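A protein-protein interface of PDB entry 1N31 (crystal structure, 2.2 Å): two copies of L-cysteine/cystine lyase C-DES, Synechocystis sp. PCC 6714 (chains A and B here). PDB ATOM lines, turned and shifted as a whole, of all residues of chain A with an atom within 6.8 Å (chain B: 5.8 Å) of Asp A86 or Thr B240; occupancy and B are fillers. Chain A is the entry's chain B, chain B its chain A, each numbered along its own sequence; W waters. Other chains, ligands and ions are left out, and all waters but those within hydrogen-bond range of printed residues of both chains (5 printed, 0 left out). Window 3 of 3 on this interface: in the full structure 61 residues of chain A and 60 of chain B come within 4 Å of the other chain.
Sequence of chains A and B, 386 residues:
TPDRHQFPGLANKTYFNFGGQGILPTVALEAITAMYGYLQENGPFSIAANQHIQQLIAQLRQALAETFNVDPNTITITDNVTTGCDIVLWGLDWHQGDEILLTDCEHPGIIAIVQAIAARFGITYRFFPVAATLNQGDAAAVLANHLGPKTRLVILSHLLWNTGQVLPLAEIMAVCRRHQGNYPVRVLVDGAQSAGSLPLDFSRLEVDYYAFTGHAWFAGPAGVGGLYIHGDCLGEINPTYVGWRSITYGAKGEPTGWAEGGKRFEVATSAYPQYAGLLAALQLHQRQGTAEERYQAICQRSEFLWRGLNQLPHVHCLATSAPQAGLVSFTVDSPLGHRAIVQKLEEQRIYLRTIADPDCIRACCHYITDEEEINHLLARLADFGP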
ATOM      1  N   ASN A  80       8.179   7.005  22.423  1.00  0.00           N
ATOM      2  CA  ASN A  80       6.885   7.016  21.776  1.00  0.00           C
ATOM      3  C   ASN A  80       6.888   6.016  20.617  1.00  0.00           C
ATOM      4  O   ASN A  80       7.917   5.413  20.323  1.00  0.00           O
ATOM      5  CB  ASN A  80       6.635   8.437  21.251  1.00  0.00           C
ATOM      6  CG  ASN A  80       7.835   8.975  20.463  1.00  0.00           C
ATOM      7  OD1 ASN A  80       8.351   8.302  19.559  1.00  0.00           O
ATOM      8  ND2 ASN A  80       8.279  10.170  20.797  1.00  0.00           N
ATOM      9  N   VAL A  81       5.743   5.850  19.954  1.00  0.00           N
ATOM     10  CA  VAL A  81       5.631   4.904  18.835  1.00  0.00           C
ATOM     11  C   VAL A  81       6.534   5.245  17.671  1.00  0.00           C
ATOM     12  O   VAL A  81       7.211   4.368  17.110  1.00  0.00           O
ATOM     13  CB  VAL A  81       4.189   4.843  18.260  1.00  0.00           C
ATOM     14  CG1 VAL A  81       4.123   3.847  17.112  1.00  0.00           C
ATOM     15  CG2 VAL A  81       3.198   4.444  19.344  1.00  0.00           C
ATOM     16  N   THR A  82       6.543   6.524  17.307  1.00  0.00           N
ATOM     17  CA  THR A  82       7.285   6.960  16.143  1.00  0.00           C
ATOM     18  C   THR A  82       8.772   6.643  16.137  1.00  0.00           C
ATOM     19  O   THR A  82       9.312   6.223  15.113  1.00  0.00           O
ATOM     20  CB  THR A  82       7.063   8.468  15.894  1.00  0.00           C
ATOM     21  OG1 THR A  82       5.663   8.710  15.739  1.00  0.00           O
ATOM     22  CG2 THR A  82       7.798   8.917  14.622  1.00  0.00           C
ATOM     23  N   THR A  83       9.428   6.876  17.265  1.00  0.00           N
ATOM     24  CA  THR A  83      10.850   6.589  17.401  1.00  0.00           C
ATOM     25  C   THR A  83      11.143   5.127  17.057  1.00  0.00           C
ATOM     26  O   THR A  83      12.132   4.823  16.375  1.00  0.00           O
ATOM     27  CB  THR A  83      11.325   6.889  18.828  1.00  0.00           C
ATOM     28  OG1 THR A  83      11.148   8.279  19.090  1.00  0.00           O
ATOM     29  CG2 THR A  83      12.788   6.519  18.993  1.00  0.00           C
ATOM     30  N   GLY A  84      10.289   4.219  17.525  1.00  0.00           N
ATOM     31  CA  GLY A  84      10.474   2.810  17.186  1.00  0.00           C
ATOM     32  C   GLY A  84      10.511   2.619  15.670  1.00  0.00           C
ATOM     33  O   GLY A  84      11.356   1.872  15.144  1.00  0.00           O
ATOM     34  N   CYS A  85       9.600   3.296  14.962  1.00  0.00           N
ATOM     35  CA  CYS A  85       9.546   3.227  13.507  1.00  0.00           C
ATOM     36  C   CYS A  85      10.803   3.845  12.877  1.00  0.00           C
ATOM     37  O   CYS A  85      11.318   3.327  11.886  1.00  0.00           O
ATOM     38  CB  CYS A  85       8.285   3.947  12.969  1.00  0.00           C
ATOM     39  SG  CYS A  85       6.696   3.135  13.410  1.00  0.00           S
ATOM     40  N   ASP A  86      11.283   4.958  13.428  1.00  0.00           N
ATOM     41  CA  ASP A  86      12.518   5.594  12.924  1.00  0.00           C
ATOM     42  C   ASP A  86      13.718   4.625  13.064  1.00  0.00           C
ATOM     43  O   ASP A  86      14.581   4.551  12.173  1.00  0.00           O
ATOM     44  CB  ASP A  86      12.841   6.872  13.706  1.00  0.00           C
ATOM     45  CG  ASP A  86      12.145   8.098  13.153  1.00  0.00           C
ATOM     46  OD1 ASP A  86      12.502   8.515  12.026  1.00  0.00           O
ATOM     47  OD2 ASP A  86      11.263   8.663  13.851  1.00  0.00           O
ATOM     48  N   ILE A  87      13.761   3.894  14.178  1.00  0.00           N
ATOM     49  CA  ILE A  87      14.849   2.944  14.419  1.00  0.00           C
ATOM     50  C   ILE A  87      14.917   1.862  13.326  1.00  0.00           C
ATOM     51  O   ILE A  87      15.976   1.590  12.753  1.00  0.00           O
ATOM     52  CB  ILE A  87      14.712   2.248  15.816  1.00  0.00           C
ATOM     53  CG1 ILE A  87      15.068   3.240  16.940  1.00  0.00           C
ATOM     54  CG2 ILE A  87      15.646   1.009  15.884  1.00  0.00           C
ATOM     55  CD1 ILE A  87      14.734   2.752  18.360  1.00  0.00           C
ATOM     56  N   VAL A  88      13.781   1.253  13.036  1.00  0.00           N
ATOM     57  CA  VAL A  88      13.733   0.205  12.032  1.00  0.00           C
ATOM     58  C   VAL A  88      14.038   0.736  10.633  1.00  0.00           C
ATOM     59  O   VAL A  88      14.901   0.207   9.934  1.00  0.00           O
ATOM     60  CB  VAL A  88      12.342  -0.493  12.022  1.00  0.00           C
ATOM     61  CG1 VAL A  88      12.312  -1.562  10.935  1.00  0.00           C
ATOM     62  CG2 VAL A  88      12.058  -1.131  13.400  1.00  0.00           C
ATOM     63  N   LEU A  89      13.338   1.792  10.244  1.00  0.00           N
ATOM     64  CA  LEU A  89      13.503   2.384   8.925  1.00  0.00           C
ATOM     65  C   LEU A  89      14.908   2.903   8.617  1.00  0.00           C
ATOM     66  O   LEU A  89      15.460   2.635   7.544  1.00  0.00           O
ATOM     67  CB  LEU A  89      12.461   3.488   8.723  1.00  0.00           C
ATOM     68  CG  LEU A  89      11.021   2.939   8.656  1.00  0.00           C
ATOM     69  CD1 LEU A  89      10.037   4.083   8.731  1.00  0.00           C
ATOM     70  CD2 LEU A  89      10.819   2.136   7.375  1.00  0.00           C
ATOM     71  N   TRP A  90      15.491   3.656   9.535  1.00  0.00           N
ATOM     72  CA  TRP A  90      16.832   4.163   9.294  1.00  0.00           C
ATOM     73  C   TRP A  90      17.892   3.087   9.486  1.00  0.00           C
ATOM     74  O   TRP A  90      19.006   3.237   9.023  1.00  0.00           O
ATOM     75  CB  TRP A  90      17.122   5.346  10.206  1.00  0.00           C
ATOM     76  CG  TRP A  90      16.425   6.560   9.744  1.00  0.00           C
ATOM     77  CD1 TRP A  90      15.275   7.093  10.253  1.00  0.00           C
ATOM     78  CD2 TRP A  90      16.832   7.429   8.672  1.00  0.00           C
ATOM     79  NE1 TRP A  90      14.950   8.244   9.568  1.00  0.00           N
ATOM     80  CE2 TRP A  90      15.887   8.470   8.596  1.00  0.00           C
ATOM     81  CE3 TRP A  90      17.906   7.424   7.773  1.00  0.00           C
ATOM     82  CZ2 TRP A  90      15.983   9.502   7.654  1.00  0.00           C
ATOM     83  CZ3 TRP A  90      18.006   8.454   6.833  1.00  0.00           C
ATOM     84  CH2 TRP A  90      17.055   9.477   6.781  1.00  0.00           C
ATOM     85  N   GLY A  91      17.532   1.990  10.141  1.00  0.00           N
ATOM     86  CA  GLY A  91      18.495   0.919  10.368  1.00  0.00           C
ATOM     87  C   GLY A  91      18.730  -0.048   9.200  1.00  0.00           C
ATOM     88  O   GLY A  91      19.800  -0.645   9.090  1.00  0.00           O
ATOM     89  N   GLY A 109       2.974  10.971  10.410  1.00  0.00           N
ATOM     90  CA  GLY A 109       4.339  11.024  10.910  1.00  0.00           C
ATOM     91  C   GLY A 109       5.193   9.912  10.316  1.00  0.00           C
ATOM     92  O   GLY A 109       6.344  10.131   9.958  1.00  0.00           O
ATOM     93  N   ALA A 112       6.046  10.471   6.706  1.00  0.00           N
ATOM     94  CA  ALA A 112       7.111  11.465   6.627  1.00  0.00           C
ATOM     95  C   ALA A 112       8.501  10.840   6.736  1.00  0.00           C
ATOM     96  O   ALA A 112       9.470  11.335   6.133  1.00  0.00           O
ATOM     97  CB  ALA A 112       6.933  12.500   7.709  1.00  0.00           C
ATOM     98  N   ILE A 113       8.609   9.761   7.506  1.00  0.00           N
ATOM     99  CA  ILE A 113       9.897   9.092   7.666  1.00  0.00           C
ATOM    100  C   ILE A 113      10.222   8.442   6.336  1.00  0.00           C
ATOM    101  O   ILE A 113      11.321   8.605   5.814  1.00  0.00           O
ATOM    102  CB  ILE A 113       9.852   7.972   8.734  1.00  0.00           C
ATOM    103  CG1 ILE A 113       9.517   8.556  10.100  1.00  0.00           C
ATOM    104  CG2 ILE A 113      11.214   7.260   8.801  1.00  0.00           C
ATOM    105  CD1 ILE A 113       9.378   7.485  11.204  1.00  0.00           C
ATOM    106  N   ALA A 116      11.512  10.748   3.847  1.00  0.00           N
ATOM    107  CA  ALA A 116      12.886  11.106   4.158  1.00  0.00           C
ATOM    108  C   ALA A 116      13.817   9.986   3.697  1.00  0.00           C
ATOM    109  O   ALA A 116      14.866  10.249   3.127  1.00  0.00           O
ATOM    110  CB  ALA A 116      13.032  11.344   5.652  1.00  0.00           C
ATOM    111  N   ILE A 117      13.427   8.736   3.929  1.00  0.00           N
ATOM    112  CA  ILE A 117      14.252   7.606   3.527  1.00  0.00           C
ATOM    113  C   ILE A 117      14.375   7.560   2.012  1.00  0.00           C
ATOM    114  O   ILE A 117      15.477   7.413   1.478  1.00  0.00           O
ATOM    115  CB  ILE A 117      13.659   6.263   3.990  1.00  0.00           C
ATOM    116  CG1 ILE A 117      13.628   6.187   5.528  1.00  0.00           C
ATOM    117  CG2 ILE A 117      14.475   5.107   3.410  1.00  0.00           C
ATOM    118  CD1 ILE A 117      14.958   6.281   6.174  1.00  0.00           C
ATOM    119  N   ARG A 120      16.786   9.855   0.725  1.00  0.00           N
ATOM    120  CA  ARG A 120      18.178   9.584   1.147  1.00  0.00           C
ATOM    121  C   ARG A 120      18.828   8.379   0.453  1.00  0.00           C
ATOM    122  O   ARG A 120      20.008   8.410   0.120  1.00  0.00           O
ATOM    123  CB  ARG A 120      18.248   9.341   2.670  1.00  0.00           C
ATOM    124  CG  ARG A 120      19.517   9.884   3.343  1.00  0.00           C
ATOM    125  CD  ARG A 120      19.415  11.391   3.511  1.00  0.00           C
ATOM    126  NE  ARG A 120      18.879  11.797   4.812  1.00  0.00           N
ATOM    127  CZ  ARG A 120      19.559  11.766   5.957  1.00  0.00           C
ATOM    128  NH1 ARG A 120      20.812  11.338   5.980  1.00  0.00           N
ATOM    129  NH2 ARG A 120      18.996  12.198   7.078  1.00  0.00           N
ATOM    130  N   LEU A 188       6.920  -4.103   9.242  1.00  0.00           N
ATOM    131  CA  LEU A 188       7.030  -3.230  10.420  1.00  0.00           C
ATOM    132  C   LEU A 188       5.590  -2.897  10.846  1.00  0.00           C
ATOM    133  O   LEU A 188       4.825  -2.323  10.062  1.00  0.00           O
ATOM    134  CB  LEU A 188       7.767  -1.937  10.047  1.00  0.00           C
ATOM    135  CG  LEU A 188       7.606  -0.736  10.993  1.00  0.00           C
ATOM    136  CD1 LEU A 188       8.163  -1.046  12.396  1.00  0.00           C
ATOM    137  CD2 LEU A 188       8.335   0.445  10.392  1.00  0.00           C
ATOM    138  N   THR A 240      21.429   3.755  14.499  1.00  0.00           N
ATOM    139  CA  THR A 240      21.527   5.034  13.818  1.00  0.00           C
ATOM    140  C   THR A 240      21.764   6.075  14.903  1.00  0.00           C
ATOM    141  O   THR A 240      22.906   6.478  15.136  1.00  0.00           O
ATOM    142  CB  THR A 240      20.216   5.340  13.059  1.00  0.00           C
ATOM    143  OG1 THR A 240      19.995   4.323  12.078  1.00  0.00           O
ATOM    144  CG2 THR A 240      20.306   6.669  12.330  1.00  0.00           C
ATOM    145  N   TYR A 241      20.705   6.534  15.565  1.00  0.00           N
ATOM    146  CA  TYR A 241      20.924   7.473  16.670  1.00  0.00           C
ATOM    147  C   TYR A 241      21.475   6.664  17.841  1.00  0.00           C
ATOM    148  O   TYR A 241      20.801   5.784  18.373  1.00  0.00           O
ATOM    149  CB  TYR A 241      19.620   8.153  17.111  1.00  0.00           C
ATOM    150  CG  TYR A 241      19.233   9.373  16.314  1.00  0.00           C
ATOM    151  CD1 TYR A 241      18.413  10.345  16.873  1.00  0.00           C
ATOM    152  CD2 TYR A 241      19.612   9.515  14.986  1.00  0.00           C
ATOM    153  CE1 TYR A 241      17.969  11.420  16.129  1.00  0.00           C
ATOM    154  CE2 TYR A 241      19.172  10.582  14.225  1.00  0.00           C
ATOM    155  CZ  TYR A 241      18.342  11.540  14.801  1.00  0.00           C
ATOM    156  OH  TYR A 241      17.863  12.612  14.050  1.00  0.00           O
ATOM    157  N   ASP B  86      23.477  13.721  17.384  1.00  0.00           N
ATOM    158  CA  ASP B  86      22.984  12.759  16.379  1.00  0.00           C
ATOM    159  C   ASP B  86      22.303  13.482  15.230  1.00  0.00           C
ATOM    160  O   ASP B  86      22.451  13.104  14.055  1.00  0.00           O
ATOM    161  CB  ASP B  86      21.986  11.779  16.995  1.00  0.00           C
ATOM    162  CG  ASP B  86      22.659  10.585  17.651  1.00  0.00           C
ATOM    163  OD1 ASP B  86      23.256   9.761  16.919  1.00  0.00           O
ATOM    164  OD2 ASP B  86      22.580  10.479  18.893  1.00  0.00           O
ATOM    165  N   ILE B  87      21.556  14.531  15.570  1.00  0.00           N
ATOM    166  CA  ILE B  87      20.843  15.319  14.560  1.00  0.00           C
ATOM    167  C   ILE B  87      21.796  15.956  13.546  1.00  0.00           C
ATOM    168  O   ILE B  87      21.564  15.880  12.340  1.00  0.00           O
ATOM    169  CB  ILE B  87      19.965  16.441  15.219  1.00  0.00           C
ATOM    170  CG1 ILE B  87      18.714  15.824  15.843  1.00  0.00           C
ATOM    171  CG2 ILE B  87      19.577  17.480  14.178  1.00  0.00           C
ATOM    172  CD1 ILE B  87      17.971  16.758  16.808  1.00  0.00           C
ATOM    173  N   TRP B  90      24.003  12.899  11.623  1.00  0.00           N
ATOM    174  CA  TRP B  90      23.251  12.140  10.634  1.00  0.00           C
ATOM    175  C   TRP B  90      22.618  13.025   9.569  1.00  0.00           C
ATOM    176  O   TRP B  90      22.210  12.550   8.509  1.00  0.00           O
ATOM    177  CB  TRP B  90      22.156  11.300  11.299  1.00  0.00           C
ATOM    178  CG  TRP B  90      22.690  10.118  11.983  1.00  0.00           C
ATOM    179  CD1 TRP B  90      22.945   9.987  13.320  1.00  0.00           C
ATOM    180  CD2 TRP B  90      23.100   8.894  11.371  1.00  0.00           C
ATOM    181  NE1 TRP B  90      23.492   8.761  13.580  1.00  0.00           N
ATOM    182  CE2 TRP B  90      23.598   8.060  12.405  1.00  0.00           C
ATOM    183  CE3 TRP B  90      23.095   8.414  10.051  1.00  0.00           C
ATOM    184  CZ2 TRP B  90      24.090   6.766  12.162  1.00  0.00           C
ATOM    185  CZ3 TRP B  90      23.588   7.116   9.809  1.00  0.00           C
ATOM    186  CH2 TRP B  90      24.075   6.314  10.859  1.00  0.00           C
ATOM    187  N   GLY B  91      22.540  14.318   9.834  1.00  0.00           N
ATOM    188  CA  GLY B  91      21.912  15.207   8.873  1.00  0.00           C
ATOM    189  C   GLY B  91      22.786  15.716   7.736  1.00  0.00           C
ATOM    190  O   GLY B  91      22.265  16.110   6.700  1.00  0.00           O
ATOM    191  N   ASN B 238      19.857  17.654   6.894  1.00  0.00           N
ATOM    192  CA  ASN B 238      18.655  16.962   6.459  1.00  0.00           C
ATOM    193  C   ASN B 238      18.015  16.276   7.683  1.00  0.00           C
ATOM    194  O   ASN B 238      18.700  15.627   8.457  1.00  0.00           O
ATOM    195  CB  ASN B 238      19.017  15.892   5.407  1.00  0.00           C
ATOM    196  CG  ASN B 238      19.670  16.483   4.130  1.00  0.00           C
ATOM    197  OD1 ASN B 238      19.013  17.164   3.345  1.00  0.00           O
ATOM    198  ND2 ASN B 238      20.964  16.211   3.930  1.00  0.00           N
ATOM    199  N   PRO B 239      16.690  16.421   7.875  1.00  0.00           N
ATOM    200  CA  PRO B 239      16.065  15.763   9.033  1.00  0.00           C
ATOM    201  C   PRO B 239      16.278  14.265   8.855  1.00  0.00           C
ATOM    202  O   PRO B 239      16.294  13.793   7.732  1.00  0.00           O
ATOM    203  CB  PRO B 239      14.585  16.152   8.899  1.00  0.00           C
ATOM    204  CG  PRO B 239      14.637  17.507   8.252  1.00  0.00           C
ATOM    205  CD  PRO B 239      15.738  17.330   7.197  1.00  0.00           C
ATOM    206  N   THR B 240      16.446  13.536   9.953  1.00  0.00           N
ATOM    207  CA  THR B 240      16.667  12.093   9.919  1.00  0.00           C
ATOM    208  C   THR B 240      15.533  11.448  10.722  1.00  0.00           C
ATOM    209  O   THR B 240      14.575  10.943  10.137  1.00  0.00           O
ATOM    210  CB  THR B 240      18.047  11.739  10.530  1.00  0.00           C
ATOM    211  OG1 THR B 240      19.084  12.352   9.746  1.00  0.00           O
ATOM    212  CG2 THR B 240      18.267  10.228  10.521  1.00  0.00           C
ATOM    213  N   TYR B 241      15.623  11.454  12.056  1.00  0.00           N
ATOM    214  CA  TYR B 241      14.514  10.919  12.836  1.00  0.00           C
ATOM    215  C   TYR B 241      13.432  11.982  12.839  1.00  0.00           C
ATOM    216  O   TYR B 241      13.614  13.061  13.397  1.00  0.00           O
ATOM    217  CB  TYR B 241      14.897  10.613  14.279  1.00  0.00           C
ATOM    218  CG  TYR B 241      15.561   9.269  14.514  1.00  0.00           C
ATOM    219  CD1 TYR B 241      15.503   8.666  15.772  1.00  0.00           C
ATOM    220  CD2 TYR B 241      16.326   8.645  13.516  1.00  0.00           C
ATOM    221  CE1 TYR B 241      16.185   7.501  16.042  1.00  0.00           C
ATOM    222  CE2 TYR B 241      17.020   7.469  13.781  1.00  0.00           C
ATOM    223  CZ  TYR B 241      16.945   6.906  15.048  1.00  0.00           C
ATOM    224  OH  TYR B 241      17.632   5.743  15.329  1.00  0.00           O
ATOM    225  N   VAL B 242      12.307  11.685  12.197  1.00  0.00           N
ATOM    226  CA  VAL B 242      11.200  12.628  12.145  1.00  0.00           C
ATOM    227  C   VAL B 242       9.901  11.958  12.581  1.00  0.00           C
ATOM    228  O   VAL B 242       9.834  10.735  12.778  1.00  0.00           O
ATOM    229  CB  VAL B 242      10.996  13.178  10.706  1.00  0.00           C
ATOM    230  CG1 VAL B 242      12.187  14.062  10.293  1.00  0.00           C
ATOM    231  CG2 VAL B 242      10.834  12.007   9.718  1.00  0.00           C
ATOM    232  N   GLY B 243       8.863  12.780  12.685  1.00  0.00           N
ATOM    233  CA  GLY B 243       7.543  12.316  13.081  1.00  0.00           C
ATOM    234  C   GLY B 243       6.481  13.389  12.860  1.00  0.00           C
ATOM    235  O   GLY B 243       6.698  14.328  12.083  1.00  0.00           O
ATOM    236  N   PHE B 265      13.297  18.914  13.432  1.00  0.00           N
ATOM    237  CA  PHE B 265      14.105  17.849  14.031  1.00  0.00           C
ATOM    238  C   PHE B 265      13.464  17.296  15.316  1.00  0.00           C
ATOM    239  O   PHE B 265      14.092  16.528  16.042  1.00  0.00           O
ATOM    240  CB  PHE B 265      15.532  18.347  14.325  1.00  0.00           C
ATOM    241  CG  PHE B 265      16.234  18.946  13.112  1.00  0.00           C
ATOM    242  CD1 PHE B 265      16.554  20.310  13.077  1.00  0.00           C
ATOM    243  CD2 PHE B 265      16.524  18.153  11.994  1.00  0.00           C
ATOM    244  CE1 PHE B 265      17.156  20.885  11.934  1.00  0.00           C
ATOM    245  CE2 PHE B 265      17.123  18.711  10.842  1.00  0.00           C
ATOM    246  CZ  PHE B 265      17.439  20.081  10.814  1.00  0.00           C
ATOM    247  N   VAL B 267      10.595  14.971  17.038  1.00  0.00           N
ATOM    248  CA  VAL B 267       9.895  13.788  16.541  1.00  0.00           C
ATOM    249  C   VAL B 267       8.426  13.569  16.872  1.00  0.00           C
ATOM    250  O   VAL B 267       7.581  13.611  15.973  1.00  0.00           O
ATOM    251  CB  VAL B 267      10.674  12.525  16.940  1.00  0.00           C
ATOM    252  CG1 VAL B 267       9.985  11.286  16.397  1.00  0.00           C
ATOM    253  CG2 VAL B 267      12.109  12.639  16.465  1.00  0.00           C
HETATM  254  O   HOH W   1      18.194   5.344  18.198  1.00  0.00           O
HETATM  255  O   HOH W   2      19.136   3.501  16.346  1.00  0.00           O
HETATM  256  O   HOH W   3      16.495  14.812  12.545  1.00  0.00           O
HETATM  257  O   HOH W   4      15.357  14.270  14.884  1.00  0.00           O
HETATM  258  O   HOH W   5      23.020  12.693   5.130  1.00  0.00           O
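O of Trp B90 lies within hydrogen-bond range of NH1 of Arg A120, at 3.1 Å.
The backbone carbonyl oxygen (O) of Thr A240 lies within hydrogen-bond range of the indole nitrogen (NE1) of Trp B90 (2.8 Å).
O of Pro B239 is in hydrogen-bond range of NH2 of Arg A120 (3.2 Å).
O of Thr B240 is in hydrogen-bond range of NE1 of Trp A90 (2.8 Å).
The guanidinium group of Arg A120 is in hydrogen-bond range of the side-chain hydroxyl of Thr B240, 2.7 Å away.
N of Tyr A241 lies within hydrogen-bond range of OH of Tyr B241 (3.2 Å).
The side-chain carboxylate (OD1) of Asp A86 sits at hydrogen-bond distance from the backbone NH (N) of Val B242.
The side-chain carboxylate (OD1) of Asp B86 lies within hydrogen-bond range of the indole nitrogen (NE1) of Trp B90.
O of Trp B90 is in hydrogen-bond range of OG1 of Thr B240, at 3.4 Å.
The backbone carbonyl oxygen of Gly B91 is in hydrogen-bond range of the backbone NH of Asn B238, 2.9 Å away.
The side-chain amide oxygen (OD1) of Asn A80 lies close to the backbone NH (N) of Thr A82.
NE1 of Trp A90 lies within hydrogen-bond range of OD1 of Asp A86 (3.5 Å).
The side-chain hydroxyl (OG1) of Thr A240 lies within hydrogen-bond range of the backbone carbonyl oxygen (O) of Trp A90 (3.4 Å).
Thr A82 touches Val B267.
Asp A86 touches Thr B240 (OD1 to O, 3.7 Å).
Asp A86 touches Tyr B241.
CG1 of Ile A87 touches OH of Tyr B241 (3.9 Å).
Gly A109 touches Gly B243.
Val B242 touches Ala A112 (CG2 to O, 3.9 Å).
Arg A120 touches Asn B238.
Asp B86 touches Tyr A241 (OD1 to CA, 3.3 Å).
Trp B90 touches Tyr A241 (CD1 to CD2, 3.8 Å).
Thr B240 touches Tyr A241 (CB to OH, 3.6 Å).
Asp A86 touches just these residues of chain B: Thr B240 (3.7 Å), Tyr B241 (3.2 Å), Val B242 (2.7 Å) and Val B267 (3.9 Å).
Of the printed residues of chain B, Ile A113 touches Val B242 (3.5 Å).
Of the printed residues of chain A, Asp B86 touches Thr A240 (3.8 Å) and Tyr A241 (3.3 Å).
Printed residues of chain A within 4 Å of Ile B87: Tyr A241 (3.8 Å).
Of chain A, only Asp A86, Trp A90, Arg A120 and Tyr A241 come within 4 Å of Thr B240.
Of the printed residues of chain A, Val B242 touches Thr A82, Asp A86, Ala A112 and Ile A113.
The nearest residue of chain B that does not touch Asp A86 is Gly B243 (4.9 Å).
The nearest residue of chain A that does not touch Thr B240 is Thr A240 (4.5 Å).
The nearest printed residue of chain A that does not touch Val B267 is Thr A83 (4.2 Å).
Printed residues of chain A that touch a printed residue of chain B: Thr A82, Asp A86, Ile A87, Trp A90, Gly A109, Ala A112, Ile A113, Arg A120, Thr A240 and Tyr A241.
Of the 12 printed residues of chain B, 10 touch a printed residue of chain A.
Printed residues of chain B that touch a printed residue of chain A: Asp B86, Ile B87, Trp B90, Asn B238, Pro B239, Thr B240, Tyr B241, Val B242, Gly B243 and Val B267.
Hydrophobic or aromatic side chains of chain B that line the printed part of chain A: Ile B87, Trp B90, Tyr B241, Val B242 and Val B267.
Among the printed residues, no Asp or Glu carboxylate lies within 4 Å of a Lys or Arg side-chain nitrogen of the other chain.
Asp A86 touches Thr B240, and with the chains exchanged Thr A240 touches Asp B86.
Ile A87 touches Tyr B241, and with the chains exchanged Tyr A241 touches Ile B87.
Trp A90 touches Thr B240, and with the chains exchanged Thr A240 touches Trp B90.
Tyr A241 touches its own counterpart, Tyr B241.
Water W4 lies within hydrogen-bond range of the backbone carbonyl oxygen (O) of Tyr B241, the backbone carbonyl oxygen (O) of Phe B265 and the side-chain hydroxyl (OH) of Tyr A241.
Water W1 bridges O of Tyr A241 (2.6 Å) and OH of Tyr B241 (3.0 Å).
Water W5 bridges the guanidinium group (NH1) of Arg A120 (2.7 Å) and the backbone carbonyl oxygen (O) of Trp B90 (3.5 Å).
Water W2 lies within hydrogen-bond range of OH of Tyr B241, N of Thr A240 and O of Tyr A241.
Water W3 lies within hydrogen-bond range of the backbone NH (N) of Thr B240 (2.9 Å), the side-chain hydroxyl (OH) of Tyr A241 (3.0 Å) and the backbone carbonyl oxygen (O) of Tyr B241 (3.5 Å).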
